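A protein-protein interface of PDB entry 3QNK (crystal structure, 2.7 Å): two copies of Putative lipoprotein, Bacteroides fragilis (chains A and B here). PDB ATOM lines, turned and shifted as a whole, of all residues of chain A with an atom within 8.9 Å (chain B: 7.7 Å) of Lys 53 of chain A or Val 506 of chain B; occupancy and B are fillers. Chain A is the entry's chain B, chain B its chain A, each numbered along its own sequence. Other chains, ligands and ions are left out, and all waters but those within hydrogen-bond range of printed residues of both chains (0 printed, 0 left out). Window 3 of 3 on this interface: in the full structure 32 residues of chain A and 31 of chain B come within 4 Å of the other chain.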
ATOM      1  N   SER A  48     -35.762 -15.109   9.979  1.00  0.00           N
ATOM      2  CA  SER A  48     -34.750 -14.132   9.530  1.00  0.00           C
ATOM      3  C   SER A  48     -33.852 -14.649   8.401  1.00  0.00           C
ATOM      4  O   SER A  48     -33.425 -15.804   8.417  1.00  0.00           O
ATOM      5  CB  SER A  48     -33.856 -13.710  10.697  1.00  0.00           C
ATOM      6  OG  SER A  48     -32.898 -12.724  10.347  1.00  0.00           O
ATOM      7  N   ALA A  49     -33.509 -13.757   7.462  1.00  0.00           N
ATOM      8  CA  ALA A  49     -32.539 -14.032   6.407  1.00  0.00           C
ATOM      9  C   ALA A  49     -31.154 -14.299   7.053  1.00  0.00           C
ATOM     10  O   ALA A  49     -30.228 -14.767   6.360  1.00  0.00           O
ATOM     11  CB  ALA A  49     -32.462 -12.847   5.456  1.00  0.00           C
ATOM     12  N   GLN A  50     -31.039 -14.011   8.397  1.00  0.00           N
ATOM     13  CA  GLN A  50     -29.841 -14.216   9.215  1.00  0.00           C
ATOM     14  C   GLN A  50     -29.984 -15.423  10.143  1.00  0.00           C
ATOM     15  O   GLN A  50     -29.184 -15.565  11.072  1.00  0.00           O
ATOM     16  CB  GLN A  50     -29.496 -12.976  10.048  1.00  0.00           C
ATOM     17  CG  GLN A  50     -28.856 -11.858   9.255  1.00  0.00           C
ATOM     18  CD  GLN A  50     -29.827 -11.119   8.366  1.00  0.00           C
ATOM     19  OE1 GLN A  50     -30.894 -10.592   8.800  1.00  0.00           O
ATOM     20  NE2 GLN A  50     -29.473 -11.082   7.094  1.00  0.00           N
ATOM     21  N   ARG A  51     -30.993 -16.295   9.872  1.00  0.00           N
ATOM     22  CA  ARG A  51     -31.329 -17.479  10.636  1.00  0.00           C
ATOM     23  C   ARG A  51     -30.104 -18.261  10.957  1.00  0.00           C
ATOM     24  O   ARG A  51     -29.944 -18.643  12.120  1.00  0.00           O
ATOM     25  CB  ARG A  51     -32.342 -18.363   9.887  1.00  0.00           C
ATOM     26  CG  ARG A  51     -32.708 -19.678  10.608  1.00  0.00           C
ATOM     27  CD  ARG A  51     -33.215 -20.730   9.658  1.00  0.00           C
ATOM     28  NE  ARG A  51     -32.165 -21.191   8.751  1.00  0.00           N
ATOM     29  CZ  ARG A  51     -32.393 -21.641   7.521  1.00  0.00           C
ATOM     30  NH1 ARG A  51     -33.626 -21.665   7.033  1.00  0.00           N
ATOM     31  NH2 ARG A  51     -31.387 -22.024   6.752  1.00  0.00           N
ATOM     32  N   ASP A  52     -29.220 -18.473   9.943  1.00  0.00           N
ATOM     33  CA  ASP A  52     -27.979 -19.242  10.078  1.00  0.00           C
ATOM     34  C   ASP A  52     -26.796 -18.380  10.498  1.00  0.00           C
ATOM     35  O   ASP A  52     -26.030 -18.798  11.368  1.00  0.00           O
ATOM     36  CB  ASP A  52     -27.640 -19.969   8.777  1.00  0.00           C
ATOM     37  CG  ASP A  52     -28.715 -20.932   8.270  1.00  0.00           C
ATOM     38  OD1 ASP A  52     -29.316 -21.669   9.110  1.00  0.00           O
ATOM     39  OD2 ASP A  52     -28.928 -20.986   7.028  1.00  0.00           O
ATOM     40  N   LYS A  53     -26.657 -17.186   9.902  1.00  0.00           N
ATOM     41  CA  LYS A  53     -25.550 -16.268  10.158  1.00  0.00           C
ATOM     42  C   LYS A  53     -25.480 -15.816  11.634  1.00  0.00           C
ATOM     43  O   LYS A  53     -24.372 -15.702  12.163  1.00  0.00           O
ATOM     44  CB  LYS A  53     -25.643 -15.057   9.210  1.00  0.00           C
ATOM     45  CG  LYS A  53     -24.371 -14.204   9.105  1.00  0.00           C
ATOM     46  CD  LYS A  53     -24.584 -13.017   8.174  1.00  0.00           C
ATOM     47  CE  LYS A  53     -23.324 -12.538   7.494  1.00  0.00           C
ATOM     48  NZ  LYS A  53     -23.639 -11.506   6.462  1.00  0.00           N
ATOM     49  N   TYR A  54     -26.618 -15.549  12.284  1.00  0.00           N
ATOM     50  CA  TYR A  54     -26.615 -15.078  13.682  1.00  0.00           C
ATOM     51  C   TYR A  54     -27.387 -15.993  14.635  1.00  0.00           C
ATOM     52  O   TYR A  54     -27.791 -15.549  15.714  1.00  0.00           O
ATOM     53  CB  TYR A  54     -27.176 -13.651  13.771  1.00  0.00           C
ATOM     54  CG  TYR A  54     -26.248 -12.604  13.191  1.00  0.00           C
ATOM     55  CD1 TYR A  54     -25.264 -12.010  13.971  1.00  0.00           C
ATOM     56  CD2 TYR A  54     -26.344 -12.220  11.857  1.00  0.00           C
ATOM     57  CE1 TYR A  54     -24.380 -11.075  13.430  1.00  0.00           C
ATOM     58  CE2 TYR A  54     -25.488 -11.262  11.315  1.00  0.00           C
ATOM     59  CZ  TYR A  54     -24.513 -10.684  12.108  1.00  0.00           C
ATOM     60  OH  TYR A  54     -23.670  -9.738  11.574  1.00  0.00           O
ATOM     61  N   ARG A  55     -27.530 -17.277  14.263  1.00  0.00           N
ATOM     62  CA  ARG A  55     -28.204 -18.338  15.002  1.00  0.00           C
ATOM     63  C   ARG A  55     -27.959 -18.289  16.501  1.00  0.00           C
ATOM     64  O   ARG A  55     -28.902 -18.122  17.258  1.00  0.00           O
ATOM     65  CB  ARG A  55     -27.744 -19.705  14.483  1.00  0.00           C
ATOM     66  CG  ARG A  55     -28.429 -20.876  15.173  1.00  0.00           C
ATOM     67  CD  ARG A  55     -28.065 -22.177  14.522  1.00  0.00           C
ATOM     68  NE  ARG A  55     -28.523 -22.192  13.146  1.00  0.00           N
ATOM     69  CZ  ARG A  55     -29.754 -22.513  12.790  1.00  0.00           C
ATOM     70  NH1 ARG A  55     -30.647 -22.862  13.709  1.00  0.00           N
ATOM     71  NH2 ARG A  55     -30.098 -22.510  11.515  1.00  0.00           N
ATOM     72  N   ALA A  56     -26.695 -18.438  16.905  1.00  0.00           N
ATOM     73  CA  ALA A  56     -26.274 -18.478  18.299  1.00  0.00           C
ATOM     74  C   ALA A  56     -26.400 -17.139  18.988  1.00  0.00           C
ATOM     75  O   ALA A  56     -26.749 -17.120  20.165  1.00  0.00           O
ATOM     76  CB  ALA A  56     -24.845 -18.983  18.392  1.00  0.00           C
ATOM     77  N   SER A  57     -26.104 -16.032  18.279  1.00  0.00           N
ATOM     78  CA  SER A  57     -26.168 -14.679  18.844  1.00  0.00           C
ATOM     79  C   SER A  57     -27.575 -14.180  19.061  1.00  0.00           C
ATOM     80  O   SER A  57     -27.815 -13.567  20.083  1.00  0.00           O
ATOM     81  CB  SER A  57     -25.465 -13.671  17.944  1.00  0.00           C
ATOM     82  OG  SER A  57     -24.060 -13.791  18.015  1.00  0.00           O
ATOM     83  N   TRP A  58     -28.479 -14.374  18.086  1.00  0.00           N
ATOM     84  CA  TRP A  58     -29.798 -13.775  18.093  1.00  0.00           C
ATOM     85  C   TRP A  58     -30.985 -14.695  18.247  1.00  0.00           C
ATOM     86  O   TRP A  58     -32.058 -14.181  18.589  1.00  0.00           O
ATOM     87  CB  TRP A  58     -30.023 -13.039  16.756  1.00  0.00           C
ATOM     88  CG  TRP A  58     -29.093 -11.898  16.432  1.00  0.00           C
ATOM     89  CD1 TRP A  58     -28.168 -11.320  17.254  1.00  0.00           C
ATOM     90  CD2 TRP A  58     -29.070 -11.137  15.208  1.00  0.00           C
ATOM     91  NE1 TRP A  58     -27.510 -10.305  16.588  1.00  0.00           N
ATOM     92  CE2 TRP A  58     -28.035 -10.182  15.326  1.00  0.00           C
ATOM     93  CE3 TRP A  58     -29.756 -11.242  13.979  1.00  0.00           C
ATOM     94  CZ2 TRP A  58     -27.713  -9.294  14.290  1.00  0.00           C
ATOM     95  CZ3 TRP A  58     -29.414 -10.384  12.944  1.00  0.00           C
ATOM     96  CH2 TRP A  58     -28.430  -9.400  13.117  1.00  0.00           C
ATOM     97  N   PHE A  59     -30.885 -15.993  17.861  1.00  0.00           N
ATOM     98  CA  PHE A  59     -32.132 -16.768  17.801  1.00  0.00           C
ATOM     99  C   PHE A  59     -32.215 -17.990  18.691  1.00  0.00           C
ATOM    100  O   PHE A  59     -33.067 -18.847  18.426  1.00  0.00           O
ATOM    101  CB  PHE A  59     -32.461 -17.140  16.350  1.00  0.00           C
ATOM    102  CG  PHE A  59     -32.504 -15.914  15.453  1.00  0.00           C
ATOM    103  CD1 PHE A  59     -33.374 -14.860  15.721  1.00  0.00           C
ATOM    104  CD2 PHE A  59     -31.649 -15.799  14.361  1.00  0.00           C
ATOM    105  CE1 PHE A  59     -33.388 -13.725  14.906  1.00  0.00           C
ATOM    106  CE2 PHE A  59     -31.657 -14.662  13.557  1.00  0.00           C
ATOM    107  CZ  PHE A  59     -32.507 -13.627  13.846  1.00  0.00           C
ATOM    108  N   TYR A 250     -25.619  -0.940   8.936  1.00  0.00           N
ATOM    109  CA  TYR A 250     -25.714  -2.238   9.578  1.00  0.00           C
ATOM    110  C   TYR A 250     -26.880  -2.291  10.558  1.00  0.00           C
ATOM    111  O   TYR A 250     -27.292  -3.387  10.939  1.00  0.00           O
ATOM    112  CB  TYR A 250     -24.370  -2.563  10.262  1.00  0.00           C
ATOM    113  CG  TYR A 250     -23.234  -2.767   9.274  1.00  0.00           C
ATOM    114  CD1 TYR A 250     -23.337  -3.700   8.242  1.00  0.00           C
ATOM    115  CD2 TYR A 250     -22.051  -2.037   9.377  1.00  0.00           C
ATOM    116  CE1 TYR A 250     -22.286  -3.919   7.351  1.00  0.00           C
ATOM    117  CE2 TYR A 250     -20.992  -2.248   8.486  1.00  0.00           C
ATOM    118  CZ  TYR A 250     -21.115  -3.192   7.474  1.00  0.00           C
ATOM    119  OH  TYR A 250     -20.104  -3.422   6.570  1.00  0.00           O
ATOM    120  N   TYR A 261     -31.056  -9.270  -3.395  1.00  0.00           N
ATOM    121  CA  TYR A 261     -30.701  -9.430  -4.806  1.00  0.00           C
ATOM    122  C   TYR A 261     -31.728  -8.861  -5.746  1.00  0.00           C
ATOM    123  O   TYR A 261     -32.562  -9.551  -6.332  1.00  0.00           O
ATOM    124  CB  TYR A 261     -30.387 -10.901  -5.094  1.00  0.00           C
ATOM    125  CG  TYR A 261     -29.271 -11.365  -4.193  1.00  0.00           C
ATOM    126  CD1 TYR A 261     -27.953 -10.985  -4.436  1.00  0.00           C
ATOM    127  CD2 TYR A 261     -29.544 -12.068  -3.022  1.00  0.00           C
ATOM    128  CE1 TYR A 261     -26.924 -11.367  -3.586  1.00  0.00           C
ATOM    129  CE2 TYR A 261     -28.523 -12.447  -2.154  1.00  0.00           C
ATOM    130  CZ  TYR A 261     -27.211 -12.100  -2.443  1.00  0.00           C
ATOM    131  OH  TYR A 261     -26.190 -12.483  -1.608  1.00  0.00           O
ATOM    132  N   GLY A 270     -29.061  -4.298   0.532  1.00  0.00           N
ATOM    133  CA  GLY A 270     -29.975  -4.891   1.518  1.00  0.00           C
ATOM    134  C   GLY A 270     -29.441  -6.135   2.224  1.00  0.00           C
ATOM    135  O   GLY A 270     -28.483  -6.763   1.747  1.00  0.00           O
ATOM    136  N   TRP A 271     -30.037  -6.483   3.392  1.00  0.00           N
ATOM    137  CA  TRP A 271     -29.658  -7.648   4.195  1.00  0.00           C
ATOM    138  C   TRP A 271     -30.801  -8.670   4.309  1.00  0.00           C
ATOM    139  O   TRP A 271     -30.655  -9.683   4.985  1.00  0.00           O
ATOM    140  CB  TRP A 271     -29.160  -7.249   5.610  1.00  0.00           C
ATOM    141  CG  TRP A 271     -28.090  -6.193   5.646  1.00  0.00           C
ATOM    142  CD1 TRP A 271     -28.227  -4.906   6.080  1.00  0.00           C
ATOM    143  CD2 TRP A 271     -26.739  -6.322   5.194  1.00  0.00           C
ATOM    144  NE1 TRP A 271     -27.044  -4.216   5.914  1.00  0.00           N
ATOM    145  CE2 TRP A 271     -26.112  -5.061   5.372  1.00  0.00           C
ATOM    146  CE3 TRP A 271     -25.999  -7.372   4.618  1.00  0.00           C
ATOM    147  CZ2 TRP A 271     -24.771  -4.831   5.019  1.00  0.00           C
ATOM    148  CZ3 TRP A 271     -24.668  -7.145   4.276  1.00  0.00           C
ATOM    149  CH2 TRP A 271     -24.064  -5.892   4.490  1.00  0.00           C
ATOM    150  N   LYS A 351     -28.204 -17.960  -1.519  1.00  0.00           N
ATOM    151  CA  LYS A 351     -27.322 -16.809  -1.518  1.00  0.00           C
ATOM    152  C   LYS A 351     -27.340 -16.155  -0.132  1.00  0.00           C
ATOM    153  O   LYS A 351     -28.362 -16.187   0.565  1.00  0.00           O
ATOM    154  CB  LYS A 351     -27.713 -15.794  -2.606  1.00  0.00           C
ATOM    155  CG  LYS A 351     -27.721 -16.309  -4.033  1.00  0.00           C
ATOM    156  CD  LYS A 351     -27.798 -15.145  -4.991  1.00  0.00           C
ATOM    157  CE  LYS A 351     -28.083 -15.581  -6.394  1.00  0.00           C
ATOM    158  NZ  LYS A 351     -28.252 -14.399  -7.286  1.00  0.00           N
ATOM    159  N   GLY A 352     -26.203 -15.562   0.240  1.00  0.00           N
ATOM    160  CA  GLY A 352     -26.022 -14.872   1.509  1.00  0.00           C
ATOM    161  C   GLY A 352     -26.938 -13.679   1.631  1.00  0.00           C
ATOM    162  O   GLY A 352     -26.997 -12.854   0.724  1.00  0.00           O
ATOM    163  N   ASP A 353     -27.699 -13.619   2.726  1.00  0.00           N
ATOM    164  CA  ASP A 353     -28.677 -12.574   3.048  1.00  0.00           C
ATOM    165  C   ASP A 353     -29.893 -12.569   2.064  1.00  0.00           C
ATOM    166  O   ASP A 353     -30.687 -11.631   2.066  1.00  0.00           O
ATOM    167  CB  ASP A 353     -28.027 -11.181   3.171  1.00  0.00           C
ATOM    168  CG  ASP A 353     -26.821 -11.158   4.079  1.00  0.00           C
ATOM    169  OD1 ASP A 353     -26.909 -11.731   5.215  1.00  0.00           O
ATOM    170  OD2 ASP A 353     -25.792 -10.562   3.676  1.00  0.00           O
ATOM    171  N   GLY A 354     -30.054 -13.634   1.281  1.00  0.00           N
ATOM    172  CA  GLY A 354     -31.232 -13.816   0.445  1.00  0.00           C
ATOM    173  C   GLY A 354     -32.336 -14.364   1.332  1.00  0.00           C
ATOM    174  O   GLY A 354     -32.062 -14.930   2.397  1.00  0.00           O
ATOM    175  N   LEU A 356     -34.793 -16.741   3.093  1.00  0.00           N
ATOM    176  CA  LEU A 356     -34.838 -18.178   3.323  1.00  0.00           C
ATOM    177  C   LEU A 356     -36.260 -18.714   3.181  1.00  0.00           C
ATOM    178  O   LEU A 356     -36.445 -19.922   2.947  1.00  0.00           O
ATOM    179  CB  LEU A 356     -34.282 -18.510   4.704  1.00  0.00           C
ATOM    180  CG  LEU A 356     -32.829 -18.089   4.938  1.00  0.00           C
ATOM    181  CD1 LEU A 356     -32.485 -18.177   6.403  1.00  0.00           C
ATOM    182  CD2 LEU A 356     -31.848 -18.873   4.045  1.00  0.00           C
ATOM    183  N   GLU B 143     -17.943  -0.953   4.283  1.00  0.00           N
ATOM    184  CA  GLU B 143     -17.014  -2.078   4.305  1.00  0.00           C
ATOM    185  C   GLU B 143     -15.615  -1.495   4.271  1.00  0.00           C
ATOM    186  O   GLU B 143     -14.999  -1.335   3.212  1.00  0.00           O
ATOM    187  CB  GLU B 143     -17.272  -3.081   3.170  1.00  0.00           C
ATOM    188  CG  GLU B 143     -18.489  -3.950   3.415  1.00  0.00           C
ATOM    189  CD  GLU B 143     -18.284  -5.454   3.403  1.00  0.00           C
ATOM    190  OE1 GLU B 143     -17.282  -5.931   2.821  1.00  0.00           O
ATOM    191  OE2 GLU B 143     -19.163  -6.160   3.951  1.00  0.00           O
ATOM    192  N   VAL B 500     -11.562  -9.148  18.216  1.00  0.00           N
ATOM    193  CA  VAL B 500     -12.564  -8.241  17.669  1.00  0.00           C
ATOM    194  C   VAL B 500     -13.892  -8.971  17.866  1.00  0.00           C
ATOM    195  O   VAL B 500     -13.946 -10.174  17.579  1.00  0.00           O
ATOM    196  CB  VAL B 500     -12.293  -7.890  16.176  1.00  0.00           C
ATOM    197  CG1 VAL B 500     -13.451  -7.099  15.557  1.00  0.00           C
ATOM    198  CG2 VAL B 500     -10.974  -7.149  16.012  1.00  0.00           C
ATOM    199  N   PRO B 501     -14.956  -8.318  18.390  1.00  0.00           N
ATOM    200  CA  PRO B 501     -16.244  -9.029  18.574  1.00  0.00           C
ATOM    201  C   PRO B 501     -16.739  -9.720  17.292  1.00  0.00           C
ATOM    202  O   PRO B 501     -16.672  -9.145  16.216  1.00  0.00           O
ATOM    203  CB  PRO B 501     -17.181  -7.915  19.012  1.00  0.00           C
ATOM    204  CG  PRO B 501     -16.286  -6.927  19.668  1.00  0.00           C
ATOM    205  CD  PRO B 501     -15.060  -6.911  18.828  1.00  0.00           C
ATOM    206  N   HIS B 502     -17.148 -10.983  17.412  1.00  0.00           N
ATOM    207  CA  HIS B 502     -17.572 -11.853  16.311  1.00  0.00           C
ATOM    208  C   HIS B 502     -18.615 -11.243  15.397  1.00  0.00           C
ATOM    209  O   HIS B 502     -18.500 -11.355  14.177  1.00  0.00           O
ATOM    210  CB  HIS B 502     -18.134 -13.158  16.865  1.00  0.00           C
ATOM    211  CG  HIS B 502     -18.575 -14.128  15.817  1.00  0.00           C
ATOM    212  ND1 HIS B 502     -17.654 -14.856  15.067  1.00  0.00           N
ATOM    213  CD2 HIS B 502     -19.828 -14.458  15.419  1.00  0.00           C
ATOM    214  CE1 HIS B 502     -18.378 -15.618  14.261  1.00  0.00           C
ATOM    215  NE2 HIS B 502     -19.692 -15.412  14.437  1.00  0.00           N
ATOM    216  N   ASP B 503     -19.650 -10.641  15.970  1.00  0.00           N
ATOM    217  CA  ASP B 503     -20.749 -10.068  15.192  1.00  0.00           C
ATOM    218  C   ASP B 503     -20.264  -8.937  14.286  1.00  0.00           C
ATOM    219  O   ASP B 503     -20.828  -8.738  13.206  1.00  0.00           O
ATOM    220  CB  ASP B 503     -21.887  -9.600  16.119  1.00  0.00           C
ATOM    221  CG  ASP B 503     -22.755 -10.735  16.688  1.00  0.00           C
ATOM    222  OD1 ASP B 503     -22.498 -11.925  16.343  1.00  0.00           O
ATOM    223  OD2 ASP B 503     -23.705 -10.434  17.461  1.00  0.00           O
ATOM    224  N   GLU B 504     -19.194  -8.245  14.703  1.00  0.00           N
ATOM    225  CA  GLU B 504     -18.565  -7.176  13.946  1.00  0.00           C
ATOM    226  C   GLU B 504     -17.840  -7.747  12.698  1.00  0.00           C
ATOM    227  O   GLU B 504     -17.970  -7.204  11.604  1.00  0.00           O
ATOM    228  CB  GLU B 504     -17.594  -6.425  14.861  1.00  0.00           C
ATOM    229  CG  GLU B 504     -17.443  -4.960  14.510  1.00  0.00           C
ATOM    230  CD  GLU B 504     -18.601  -4.052  14.875  1.00  0.00           C
ATOM    231  OE1 GLU B 504     -19.454  -4.458  15.701  1.00  0.00           O
ATOM    232  OE2 GLU B 504     -18.626  -2.909  14.357  1.00  0.00           O
ATOM    233  N   ILE B 505     -17.116  -8.869  12.877  1.00  0.00           N
ATOM    234  CA  ILE B 505     -16.360  -9.594  11.855  1.00  0.00           C
ATOM    235  C   ILE B 505     -17.288 -10.173  10.792  1.00  0.00           C
ATOM    236  O   ILE B 505     -16.930 -10.141   9.610  1.00  0.00           O
ATOM    237  CB  ILE B 505     -15.501 -10.734  12.504  1.00  0.00           C
ATOM    238  CG1 ILE B 505     -14.385 -10.201  13.430  1.00  0.00           C
ATOM    239  CG2 ILE B 505     -14.934 -11.714  11.471  1.00  0.00           C
ATOM    240  CD1 ILE B 505     -13.244  -9.524  12.760  1.00  0.00           C
ATOM    241  N   VAL B 506     -18.434 -10.767  11.203  1.00  0.00           N
ATOM    242  CA  VAL B 506     -19.361 -11.432  10.260  1.00  0.00           C
ATOM    243  C   VAL B 506     -20.127 -10.403   9.406  1.00  0.00           C
ATOM    244  O   VAL B 506     -20.552 -10.733   8.303  1.00  0.00           O
ATOM    245  CB  VAL B 506     -20.321 -12.466  10.907  1.00  0.00           C
ATOM    246  CG1 VAL B 506     -19.547 -13.502  11.684  1.00  0.00           C
ATOM    247  CG2 VAL B 506     -21.350 -11.817  11.798  1.00  0.00           C
ATOM    248  N   ARG B 507     -20.275  -9.175   9.933  1.00  0.00           N
ATOM    249  CA  ARG B 507     -20.931  -8.002   9.353  1.00  0.00           C
ATOM    250  C   ARG B 507     -20.202  -7.502   8.101  1.00  0.00           C
ATOM    251  O   ARG B 507     -20.846  -6.961   7.193  1.00  0.00           O
ATOM    252  CB  ARG B 507     -20.914  -6.891  10.414  1.00  0.00           C
ATOM    253  CG  ARG B 507     -21.969  -5.845  10.309  1.00  0.00           C
ATOM    254  CD  ARG B 507     -22.384  -5.329  11.679  1.00  0.00           C
ATOM    255  NE  ARG B 507     -21.565  -4.210  12.157  1.00  0.00           N
ATOM    256  CZ  ARG B 507     -21.981  -3.301  13.043  1.00  0.00           C
ATOM    257  NH1 ARG B 507     -23.206  -3.375  13.559  1.00  0.00           N
ATOM    258  NH2 ARG B 507     -21.177  -2.309  13.411  1.00  0.00           N
ATOM    259  N   SER B 508     -18.857  -7.663   8.069  1.00  0.00           N
ATOM    260  CA  SER B 508     -17.977  -7.140   7.029  1.00  0.00           C
ATOM    261  C   SER B 508     -17.037  -8.193   6.448  1.00  0.00           C
ATOM    262  O   SER B 508     -16.367  -8.915   7.194  1.00  0.00           O
ATOM    263  CB  SER B 508     -17.149  -5.993   7.611  1.00  0.00           C
ATOM    264  OG  SER B 508     -16.580  -5.142   6.631  1.00  0.00           O
ATOM    265  N   SER B 509     -16.944  -8.235   5.110  1.00  0.00           N
ATOM    266  CA  SER B 509     -16.038  -9.158   4.415  1.00  0.00           C
ATOM    267  C   SER B 509     -14.583  -8.762   4.630  1.00  0.00           C
ATOM    268  O   SER B 509     -13.728  -9.631   4.783  1.00  0.00           O
ATOM    269  CB  SER B 509     -16.315  -9.183   2.910  1.00  0.00           C
ATOM    270  OG  SER B 509     -17.678  -8.957   2.590  1.00  0.00           O
ATOM    271  N   LEU B 511     -13.346  -6.946   7.198  1.00  0.00           N
ATOM    272  CA  LEU B 511     -12.939  -6.938   8.592  1.00  0.00           C
ATOM    273  C   LEU B 511     -12.385  -8.318   8.978  1.00  0.00           C
ATOM    274  O   LEU B 511     -13.092  -9.334   8.894  1.00  0.00           O
ATOM    275  CB  LEU B 511     -14.100  -6.514   9.498  1.00  0.00           C
ATOM    276  CG  LEU B 511     -13.707  -5.897  10.837  1.00  0.00           C
ATOM    277  CD1 LEU B 511     -13.059  -4.578  10.645  1.00  0.00           C
ATOM    278  CD2 LEU B 511     -14.917  -5.674  11.701  1.00  0.00           C
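O of Asp 503 of chain B lies within hydrogen-bond range of OH of Tyr 54 of chain A, at 3.4 Å.
OG of Ser 57 of chain A is in hydrogen-bond range of OD1 of Asp 503 of chain B (3.0 Å).
OE1 of Glu 143 of chain B sits at hydrogen-bond distance from OG of Ser 509 of chain B (3.1 Å).
OE2 of Glu 504 of chain B is in salt-bridge range of NH2 of Arg 507 of chain B (2.8 Å).
The side-chain amino group of Lys 53 of chain A is in salt-bridge range of the side-chain carboxylate of Asp 353 of chain A (3.5 Å).
Val 506 of chain B touches Lys 53 of chain A (O to CE, 3.4 Å).
OH of Tyr 54 of chain A touches CG2 of Val 506 of chain B, 3.1 Å away.
Arg 507 of chain B touches Tyr 54 of chain A.
Asp 503 of chain B touches Trp 58 of chain A.
OH of Tyr 250 of chain A touches CG of Glu 143 of chain B, 3.6 Å away.
Tyr 250 of chain A touches Arg 507 of chain B.
Tyr 250 of chain A touches Ser 508 of chain B (OH to OG, 3.9 Å).
Of chain B, only Val 506 comes within 4 Å of Lys 53 of chain A.
Printed residues of chain B within 4 Å of Tyr 54 of chain A: Asp 503, Val 506 and Arg 507.
Gly 270 of chain A touches none of the printed residues of chain B.
Of the printed residues of chain A, Glu 143 of chain B touches Tyr 250 (3.6 Å).
Pro 501 of chain B touches none of the printed residues of chain A.
Of chain A, only Lys 53 and Tyr 54 come within 4 Å of Val 506 of chain B.
Printed residues of chain A within 4 Å of Ser 508 of chain B: Tyr 250 (3.9 Å).
The nearest printed residue of chain A that does not touch Ser 508 of chain B is Tyr 54 of chain A (6.3 Å).
Hydrophobic or aromatic side chains of chain A within 4 Å of the printed part of chain B: Tyr 54, Trp 58 and Tyr 250.
Along chain A the printed residues that touch a printed residue of chain B span positions 53 to 250.
Among the printed residues, no Asp or Glu carboxylate lies within 4 Å of a Lys or Arg side-chain nitrogen of the other chain.
No position is printed for both chains.
Of the 9 pairs that touch across the chains among the printed residues, none has its exchanged pair printed and touching as well.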
